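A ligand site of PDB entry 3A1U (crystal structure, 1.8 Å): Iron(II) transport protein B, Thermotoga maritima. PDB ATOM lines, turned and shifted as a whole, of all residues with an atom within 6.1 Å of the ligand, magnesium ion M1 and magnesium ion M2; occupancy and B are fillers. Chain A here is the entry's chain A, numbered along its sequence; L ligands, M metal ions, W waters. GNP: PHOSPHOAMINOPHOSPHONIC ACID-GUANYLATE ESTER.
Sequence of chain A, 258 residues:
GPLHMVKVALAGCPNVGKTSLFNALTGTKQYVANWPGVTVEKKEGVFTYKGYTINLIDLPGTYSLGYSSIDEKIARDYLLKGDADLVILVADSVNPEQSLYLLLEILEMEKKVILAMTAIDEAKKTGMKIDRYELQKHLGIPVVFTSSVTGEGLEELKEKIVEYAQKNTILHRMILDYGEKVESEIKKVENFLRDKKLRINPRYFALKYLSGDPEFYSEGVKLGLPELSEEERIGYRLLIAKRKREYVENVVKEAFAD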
ATOM      1  N   GLY A  12     -11.894 -27.241 -26.522  1.00  0.00           N
ATOM      2  CA  GLY A  12     -10.899 -26.246 -26.179  1.00  0.00           C
ATOM      3  C   GLY A  12     -10.367 -26.454 -24.775  1.00  0.00           C
ATOM      4  O   GLY A  12     -10.962 -27.200 -23.989  1.00  0.00           O
ATOM      5  N   CYS A  13      -9.242 -25.816 -24.476  1.00  0.00           N
ATOM      6  CA  CYS A  13      -8.669 -25.858 -23.128  1.00  0.00           C
ATOM      7  C   CYS A  13      -9.564 -25.122 -22.158  1.00  0.00           C
ATOM      8  O   CYS A  13     -10.418 -24.341 -22.554  1.00  0.00           O
ATOM      9  CB  CYS A  13      -7.289 -25.207 -23.138  1.00  0.00           C
ATOM     10  SG  CYS A  13      -6.136 -26.020 -24.269  1.00  0.00           S
ATOM     11  N   PRO A  14      -9.366 -25.360 -20.849  1.00  0.00           N
ATOM     12  CA  PRO A  14     -10.100 -24.570 -19.852  1.00  0.00           C
ATOM     13  C   PRO A  14      -9.987 -23.052 -20.065  1.00  0.00           C
ATOM     14  O   PRO A  14      -8.909 -22.507 -20.337  1.00  0.00           O
ATOM     15  CB  PRO A  14      -9.440 -24.983 -18.528  1.00  0.00           C
ATOM     16  CG  PRO A  14      -8.988 -26.397 -18.778  1.00  0.00           C
ATOM     17  CD  PRO A  14      -8.523 -26.402 -20.238  1.00  0.00           C
ATOM     18  N   ASN A  15     -11.136 -22.380 -19.969  1.00  0.00           N
ATOM     19  CA  ASN A  15     -11.176 -20.935 -19.876  1.00  0.00           C
ATOM     20  C   ASN A  15     -10.691 -20.165 -21.102  1.00  0.00           C
ATOM     21  O   ASN A  15     -10.148 -19.071 -20.964  1.00  0.00           O
ATOM     22  CB  ASN A  15     -10.411 -20.496 -18.623  1.00  0.00           C
ATOM     23  CG  ASN A  15     -10.971 -21.142 -17.374  1.00  0.00           C
ATOM     24  OD1 ASN A  15     -12.164 -21.119 -17.160  1.00  0.00           O
ATOM     25  ND2 ASN A  15     -10.121 -21.767 -16.586  1.00  0.00           N
ATOM     26  N   VAL A  16     -10.901 -20.713 -22.297  1.00  0.00           N
ATOM     27  CA  VAL A  16     -10.472 -20.040 -23.523  1.00  0.00           C
ATOM     28  C   VAL A  16     -11.620 -19.299 -24.191  1.00  0.00           C
ATOM     29  O   VAL A  16     -11.414 -18.586 -25.181  1.00  0.00           O
ATOM     30  CB  VAL A  16      -9.891 -21.039 -24.543  1.00  0.00           C
ATOM     31  CG1 VAL A  16      -8.603 -21.669 -24.014  1.00  0.00           C
ATOM     32  CG2 VAL A  16     -10.935 -22.099 -24.884  1.00  0.00           C
ATOM     33  N   GLY A  17     -12.830 -19.481 -23.679  1.00  0.00           N
ATOM     34  CA  GLY A  17     -13.990 -18.754 -24.173  1.00  0.00           C
ATOM     35  C   GLY A  17     -15.024 -19.599 -24.929  1.00  0.00           C
ATOM     36  O   GLY A  17     -15.802 -19.054 -25.705  1.00  0.00           O
ATOM     37  N   LYS A  18     -15.036 -20.901 -24.682  1.00  0.00           N
ATOM     38  CA  LYS A  18     -16.001 -21.804 -25.318  1.00  0.00           C
ATOM     39  C   LYS A  18     -17.435 -21.380 -25.033  1.00  0.00           C
ATOM     40  O   LYS A  18     -18.245 -21.213 -25.951  1.00  0.00           O
ATOM     41  CB  LYS A  18     -15.791 -23.250 -24.853  1.00  0.00           C
ATOM     42  CG  LYS A  18     -14.465 -23.888 -25.244  1.00  0.00           C
ATOM     43  CD  LYS A  18     -14.403 -25.348 -24.777  1.00  0.00           C
ATOM     44  CE  LYS A  18     -14.476 -25.461 -23.251  1.00  0.00           C
ATOM     45  NZ  LYS A  18     -13.372 -24.717 -22.536  1.00  0.00           N
ATOM     46  N   THR A  19     -17.754 -21.201 -23.761  1.00  0.00           N
ATOM     47  CA  THR A  19     -19.133 -20.905 -23.395  1.00  0.00           C
ATOM     48  C   THR A  19     -19.587 -19.516 -23.860  1.00  0.00           C
ATOM     49  O   THR A  19     -20.731 -19.334 -24.267  1.00  0.00           O
ATOM     50  CB  THR A  19     -19.373 -21.104 -21.898  1.00  0.00           C
ATOM     51  OG1 THR A  19     -19.134 -22.472 -21.592  1.00  0.00           O
ATOM     52  CG2 THR A  19     -20.821 -20.769 -21.543  1.00  0.00           C
ATOM     53  N   SER A  20     -18.666 -18.551 -23.839  1.00  0.00           N
ATOM     54  CA  SER A  20     -18.987 -17.221 -24.325  1.00  0.00           C
ATOM     55  C   SER A  20     -19.364 -17.276 -25.800  1.00  0.00           C
ATOM     56  O   SER A  20     -20.316 -16.626 -26.237  1.00  0.00           O
ATOM     57  CB  SER A  20     -17.827 -16.267 -24.108  1.00  0.00           C
ATOM     58  OG  SER A  20     -17.628 -16.017 -22.732  1.00  0.00           O
ATOM     59  N   LEU A  21     -18.620 -18.066 -26.561  1.00  0.00           N
ATOM     60  CA  LEU A  21     -18.913 -18.239 -27.973  1.00  0.00           C
ATOM     61  C   LEU A  21     -20.241 -18.968 -28.146  1.00  0.00           C
ATOM     62  O   LEU A  21     -21.085 -18.586 -28.970  1.00  0.00           O
ATOM     63  CB  LEU A  21     -17.782 -19.005 -28.650  1.00  0.00           C
ATOM     64  CG  LEU A  21     -17.871 -19.129 -30.177  1.00  0.00           C
ATOM     65  CD1 LEU A  21     -17.916 -17.756 -30.825  1.00  0.00           C
ATOM     66  CD2 LEU A  21     -16.697 -19.926 -30.692  1.00  0.00           C
ATOM     67  N   ASP A  58     -21.361 -27.810 -26.034  1.00  0.00           N
ATOM     68  CA  ASP A  58     -20.281 -27.097 -25.352  1.00  0.00           C
ATOM     69  C   ASP A  58     -19.514 -28.058 -24.430  1.00  0.00           C
ATOM     70  O   ASP A  58     -19.951 -28.356 -23.326  1.00  0.00           O
ATOM     71  CB  ASP A  58     -20.895 -25.941 -24.544  1.00  0.00           C
ATOM     72  CG  ASP A  58     -19.862 -25.088 -23.831  1.00  0.00           C
ATOM     73  OD1 ASP A  58     -18.661 -25.148 -24.179  1.00  0.00           O
ATOM     74  OD2 ASP A  58     -20.278 -24.331 -22.929  1.00  0.00           O
ATOM     75  N   LEU A  59     -18.353 -28.545 -24.892  1.00  0.00           N
ATOM     76  CA  LEU A  59     -17.619 -29.607 -24.202  1.00  0.00           C
ATOM     77  C   LEU A  59     -16.857 -29.111 -22.980  1.00  0.00           C
ATOM     78  O   LEU A  59     -16.505 -27.934 -22.912  1.00  0.00           O
ATOM     79  CB  LEU A  59     -16.626 -30.270 -25.159  1.00  0.00           C
ATOM     80  CG  LEU A  59     -17.239 -31.090 -26.301  1.00  0.00           C
ATOM     81  CD1 LEU A  59     -16.155 -31.660 -27.196  1.00  0.00           C
ATOM     82  CD2 LEU A  59     -18.136 -32.189 -25.736  1.00  0.00           C
ATOM     83  N   PRO A  60     -16.581 -30.016 -22.030  1.00  0.00           N
ATOM     84  CA  PRO A  60     -15.700 -29.661 -20.907  1.00  0.00           C
ATOM     85  C   PRO A  60     -14.337 -29.183 -21.417  1.00  0.00           C
ATOM     86  O   PRO A  60     -13.870 -29.665 -22.441  1.00  0.00           O
ATOM     87  CB  PRO A  60     -15.543 -30.995 -20.158  1.00  0.00           C
ATOM     88  CG  PRO A  60     -16.793 -31.761 -20.489  1.00  0.00           C
ATOM     89  CD  PRO A  60     -17.107 -31.382 -21.917  1.00  0.00           C
ATOM     90  N   GLY A  61     -13.732 -28.219 -20.721  1.00  0.00           N
ATOM     91  CA  GLY A  61     -12.383 -27.771 -21.027  1.00  0.00           C
ATOM     92  C   GLY A  61     -11.337 -28.847 -20.765  1.00  0.00           C
ATOM     93  O   GLY A  61     -11.355 -29.506 -19.713  1.00  0.00           O
ATOM     94  N   THR A  62     -10.414 -29.010 -21.698  1.00  0.00           N
ATOM     95  CA  THR A  62      -9.429 -30.089 -21.663  1.00  0.00           C
ATOM     96  C   THR A  62      -8.072 -29.617 -22.201  1.00  0.00           C
ATOM     97  O   THR A  62      -8.012 -29.075 -23.302  1.00  0.00           O
ATOM     98  CB  THR A  62      -9.892 -31.278 -22.542  1.00  0.00           C
ATOM     99  OG1 THR A  62     -10.047 -30.843 -23.897  1.00  0.00           O
ATOM    100  CG2 THR A  62     -11.233 -31.830 -22.055  1.00  0.00           C
ATOM    101  N   THR A 118     -10.411 -17.016 -30.789  1.00  0.00           N
ATOM    102  CA  THR A 118     -11.344 -16.131 -30.105  1.00  0.00           C
ATOM    103  C   THR A 118     -10.639 -15.123 -29.184  1.00  0.00           C
ATOM    104  O   THR A 118      -9.411 -15.150 -29.057  1.00  0.00           O
ATOM    105  CB  THR A 118     -12.472 -16.929 -29.379  1.00  0.00           C
ATOM    106  OG1 THR A 118     -13.633 -16.104 -29.277  1.00  0.00           O
ATOM    107  CG2 THR A 118     -12.022 -17.416 -27.985  1.00  0.00           C
ATOM    108  N   ALA A 119     -11.426 -14.237 -28.601  1.00  0.00           N
ATOM    109  CA  ALA A 119     -10.924 -13.074 -27.873  1.00  0.00           C
ATOM    110  C   ALA A 119      -9.968 -12.268 -28.751  1.00  0.00           C
ATOM    111  O   ALA A 119      -8.964 -11.735 -28.265  1.00  0.00           O
ATOM    112  CB  ALA A 119     -10.262 -13.494 -26.573  1.00  0.00           C
ATOM    113  N   ILE A 120     -10.271 -12.195 -30.035  1.00  0.00           N
ATOM    114  CA  ILE A 120      -9.419 -11.487 -30.971  1.00  0.00           C
ATOM    115  C   ILE A 120      -9.398  -9.990 -30.624  1.00  0.00           C
ATOM    116  O   ILE A 120      -8.424  -9.290 -30.912  1.00  0.00           O
ATOM    117  CB  ILE A 120      -9.841 -11.748 -32.462  1.00  0.00           C
ATOM    118  CG1 ILE A 120      -8.688 -11.425 -33.412  1.00  0.00           C
ATOM    119  CG2 ILE A 120     -11.122 -10.991 -32.822  1.00  0.00           C
ATOM    120  CD1 ILE A 120      -7.575 -12.429 -33.337  1.00  0.00           C
ATOM    121  N   ASP A 121     -10.474  -9.537 -29.991  1.00  0.00           N
ATOM    122  CA  ASP A 121     -10.555  -8.153 -29.508  1.00  0.00           C
ATOM    123  C   ASP A 121      -9.476  -7.830 -28.471  1.00  0.00           C
ATOM    124  O   ASP A 121      -8.945  -6.729 -28.441  1.00  0.00           O
ATOM    125  CB  ASP A 121     -11.936  -7.844 -28.932  1.00  0.00           C
ATOM    126  CG  ASP A 121     -12.300  -8.751 -27.768  1.00  0.00           C
ATOM    127  OD1 ASP A 121     -12.417  -9.970 -27.986  1.00  0.00           O
ATOM    128  OD2 ASP A 121     -12.442  -8.244 -26.632  1.00  0.00           O
ATOM    129  N   GLU A 122      -9.156  -8.809 -27.626  1.00  0.00           N
ATOM    130  CA  GLU A 122      -8.104  -8.642 -26.626  1.00  0.00           C
ATOM    131  C   GLU A 122      -6.738  -8.794 -27.278  1.00  0.00           C
ATOM    132  O   GLU A 122      -5.825  -8.036 -27.000  1.00  0.00           O
ATOM    133  CB  GLU A 122      -8.269  -9.655 -25.487  1.00  0.00           C
ATOM    134  N   THR A 146     -12.611 -14.587 -34.013  1.00  0.00           N
ATOM    135  CA  THR A 146     -13.887 -14.282 -33.396  1.00  0.00           C
ATOM    136  C   THR A 146     -13.759 -13.493 -32.088  1.00  0.00           C
ATOM    137  O   THR A 146     -12.759 -13.595 -31.392  1.00  0.00           O
ATOM    138  CB  THR A 146     -14.694 -15.576 -33.077  1.00  0.00           C
ATOM    139  OG1 THR A 146     -14.019 -16.327 -32.057  1.00  0.00           O
ATOM    140  CG2 THR A 146     -14.835 -16.455 -34.316  1.00  0.00           C
ATOM    141  N   SER A 147     -14.797 -12.719 -31.779  1.00  0.00           N
ATOM    142  CA  SER A 147     -14.925 -12.096 -30.463  1.00  0.00           C
ATOM    143  C   SER A 147     -16.355 -12.202 -29.966  1.00  0.00           C
ATOM    144  O   SER A 147     -17.284 -11.773 -30.644  1.00  0.00           O
ATOM    145  CB  SER A 147     -14.533 -10.618 -30.503  1.00  0.00           C
ATOM    146  OG  SER A 147     -14.788 -10.014 -29.244  1.00  0.00           O
ATOM    147  N   SER A 148     -16.508 -12.791 -28.786  1.00  0.00           N
ATOM    148  CA  SER A 148     -17.813 -12.866 -28.126  1.00  0.00           C
ATOM    149  C   SER A 148     -18.174 -11.523 -27.494  1.00  0.00           C
ATOM    150  O   SER A 148     -19.306 -11.318 -27.057  1.00  0.00           O
ATOM    151  CB  SER A 148     -17.805 -13.961 -27.054  1.00  0.00           C
ATOM    152  OG  SER A 148     -17.555 -15.222 -27.647  1.00  0.00           O
ATOM    153  N   VAL A 149     -17.200 -10.612 -27.453  1.00  0.00           N
ATOM    154  CA  VAL A 149     -17.465  -9.252 -26.964  1.00  0.00           C
ATOM    155  C   VAL A 149     -18.019  -8.351 -28.077  1.00  0.00           C
ATOM    156  O   VAL A 149     -19.101  -7.777 -27.931  1.00  0.00           O
ATOM    157  CB  VAL A 149     -16.197  -8.627 -26.355  1.00  0.00           C
ATOM    158  CG1 VAL A 149     -16.368  -7.128 -26.160  1.00  0.00           C
ATOM    159  CG2 VAL A 149     -15.870  -9.327 -25.040  1.00  0.00           C
ATOM    160  N   THR A 150     -17.283  -8.255 -29.174  1.00  0.00           N
ATOM    161  CA  THR A 150     -17.634  -7.343 -30.263  1.00  0.00           C
ATOM    162  C   THR A 150     -18.499  -7.972 -31.345  1.00  0.00           C
ATOM    163  O   THR A 150     -19.167  -7.267 -32.111  1.00  0.00           O
ATOM    164  CB  THR A 150     -16.366  -6.801 -30.951  1.00  0.00           C
ATOM    165  OG1 THR A 150     -15.753  -7.839 -31.724  1.00  0.00           O
ATOM    166  CG2 THR A 150     -15.380  -6.270 -29.920  1.00  0.00           C
HETATM  167  PG  GNP L   1     -14.403 -23.498 -19.221  1.00  0.00           P
HETATM  168  O1G GNP L   1     -14.367 -23.516 -17.729  1.00  0.00           O
HETATM  169  O2G GNP L   1     -13.315 -24.330 -19.824  1.00  0.00           O
HETATM  170  O3G GNP L   1     -15.762 -24.040 -19.492  1.00  0.00           O
HETATM  171  N3B GNP L   1     -14.326 -21.972 -19.751  1.00  0.00           N
HETATM  172  PB  GNP L   1     -14.761 -21.422 -21.187  1.00  0.00           P
HETATM  173  O1B GNP L   1     -16.168 -21.724 -21.514  1.00  0.00           O
HETATM  174  O2B GNP L   1     -13.764 -21.900 -22.179  1.00  0.00           O
HETATM  175  O3A GNP L   1     -14.603 -19.887 -21.211  1.00  0.00           O
HETATM  176  PA  GNP L   1     -15.641 -18.769 -20.902  1.00  0.00           P
HETATM  177  O1A GNP L   1     -16.222 -19.040 -19.561  1.00  0.00           O
HETATM  178  O2A GNP L   1     -16.584 -18.556 -22.011  1.00  0.00           O
HETATM  179  O5' GNP L   1     -14.813 -17.433 -20.804  1.00  0.00           O
HETATM  180  C5' GNP L   1     -13.630 -17.323 -20.011  1.00  0.00           C
HETATM  181  C4' GNP L   1     -13.315 -15.847 -19.801  1.00  0.00           C
HETATM  182  O4' GNP L   1     -12.894 -15.253 -21.055  1.00  0.00           O
HETATM  183  C3' GNP L   1     -14.511 -15.029 -19.314  1.00  0.00           C
HETATM  184  O3' GNP L   1     -14.110 -14.059 -18.348  1.00  0.00           O
HETATM  185  C2' GNP L   1     -14.990 -14.350 -20.595  1.00  0.00           C
HETATM  186  O2' GNP L   1     -15.632 -13.106 -20.352  1.00  0.00           O
HETATM  187  C1' GNP L   1     -13.687 -14.132 -21.352  1.00  0.00           C
HETATM  188  N9  GNP L   1     -13.899 -14.113 -22.793  1.00  0.00           N
HETATM  189  C8  GNP L   1     -14.484 -15.115 -23.536  1.00  0.00           C
HETATM  190  N7  GNP L   1     -14.544 -14.840 -24.813  1.00  0.00           N
HETATM  191  C5  GNP L   1     -13.976 -13.581 -24.914  1.00  0.00           C
HETATM  192  C6  GNP L   1     -13.787 -12.773 -26.044  1.00  0.00           C
HETATM  193  O6  GNP L   1     -14.091 -13.034 -27.222  1.00  0.00           O
HETATM  194  N1  GNP L   1     -13.170 -11.569 -25.732  1.00  0.00           N
HETATM  195  C2  GNP L   1     -12.806 -11.186 -24.464  1.00  0.00           C
HETATM  196  N2  GNP L   1     -12.227  -9.983 -24.357  1.00  0.00           N
HETATM  197  N3  GNP L   1     -12.977 -11.939 -23.378  1.00  0.00           N
HETATM  198  C4  GNP L   1     -13.582 -13.123 -23.677  1.00  0.00           C
HETATM  199 MG    MG M   1     -13.769 -22.257 -16.160  1.00  0.00          MG
HETATM  200 MG    MG M   2     -17.357 -23.260 -20.486  1.00  0.00          MG
HETATM  201  O   HOH W   1     -17.406 -24.893 -22.046  1.00  0.00           O
HETATM  202  O   HOH W   2     -11.160  -8.456 -22.175  1.00  0.00           O
HETATM  203  O   HOH W   3     -17.659 -21.367 -18.977  1.00  0.00           O
HETATM  204  O   HOH W   4     -18.821 -24.341 -19.168  1.00  0.00           O
HETATM  205  O   HOH W   5     -12.741 -26.117 -17.906  1.00  0.00           O
HETATM  206  O   HOH W   6     -16.154 -26.586 -19.265  1.00  0.00           O
HETATM  207  O   HOH W   7     -15.244 -16.473 -26.972  1.00  0.00           O
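O2G of the ligand is in hydrogen-bond range of N of Asn 15, 2.9 Å away. The backbone NH (N) of Ser 20 is in hydrogen-bond range of an oxygen (O2A) of the ligand. The backbone NH (N) of Val 16 sits at hydrogen-bond distance from an oxygen (O2B) of the ligand. The side-chain amino group of Lys 18 lies within salt-bridge range of an oxygen (O2G) of the ligand (2.7 Å). The side-chain carboxylate of Asp 121 sits at hydrogen-bond distance from a nitrogen (N1) of the ligand (2.9 Å). The backbone NH (N) of Ser 148 sits at hydrogen-bond distance from an oxygen (O6) of the ligand (2.9 Å). An oxygen (O2B) of the ligand sits at hydrogen-bond distance from the backbone NH (N) of Lys 18 (3.0 Å). An oxygen (O2A) of the ligand is in hydrogen-bond range of the backbone NH of Thr 19, 3.4 Å away. An oxygen (O2A) of the ligand lies within hydrogen-bond range of the side-chain hydroxyl of Ser 20, at 2.8 Å. The backbone NH (N) of Ala 119 lies within hydrogen-bond range of an oxygen (O6) of the ligand (3.2 Å). N of Gly 17 is in hydrogen-bond range of O2B of the ligand (3.0 Å).
The backbone NH (N) of Thr 150 lies within hydrogen-bond range of the side-chain hydroxyl (OG) of Ser 147 (3.1 Å). The backbone carbonyl oxygen (O) of Thr 146 lies within hydrogen-bond range of the backbone NH (N) of Ala 119, at 3.2 Å. The side-chain sulfur (SG) of Cys 13 sits close to the backbone carbonyl oxygen (O) of Thr 62, at 3.7 Å. OD2 of Asp 58 lies close to OG1 of Thr 19, at 2.6 Å. N of Val 149 lies within hydrogen-bond range of OG of Ser 147 (3.1 Å). The backbone carbonyl oxygen (O) of Cys 13 sits at hydrogen-bond distance from the side-chain amino group (NZ) of Lys 18 (3.0 Å). The side-chain carboxylate (OD1) of Asp 121 is in hydrogen-bond range of the side-chain hydroxyl (OG) of Ser 147 (2.7 Å). The side-chain hydroxyl (OG) of Ser 148 lies within hydrogen-bond range of the backbone NH (N) of Leu 21 (3.2 Å).
Cys 13 touches the ligand (O to O2G, 3.98 Å). Pro 14 touches the ligand. Gly 61 touches the ligand. OG1 of Thr 118 touches O6 of the ligand (3.7 Å). Ser 147 touches the ligand (CA to O6, 3.5 Å). Val 149 touches the ligand. Hydrophobic or aromatic side chains that line the ligand: Val 16, Ala 119 and Val 149.
The nearest printed residue that does not touch magnesium ion M1 is Pro 14 (5.5 Å).
OD2 of Asp 58 touches magnesium ion M2, at 3.96 Å. Within 4 Å of magnesium ion M2: Thr 19 and Asp 58.
O1G of the ligand is bound to magnesium ion M1 (2.1 Å). Magnesium ion M1 is bound by OD1 of Asn 15, at 2.2 Å.
Magnesium ion M2 is bound by an oxygen (O3G) of the ligand (2.0 Å), an oxygen (O1B) of the ligand (2.2 Å), the side-chain hydroxyl (OG1) of Thr 19 (2.2 Å), water W4 (2.2 Å), water W1 (2.3 Å) and water W3 (2.4 Å).
Water W1 bridges the side-chain carboxylate of Asp 58 (2.5 Å) and the backbone carbonyl oxygen of Leu 59 (3.3 Å). Water W7 lies within hydrogen-bond range of OG of Ser 148, N7 of the ligand, OG1 of Thr 118 and O of Gly 17.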
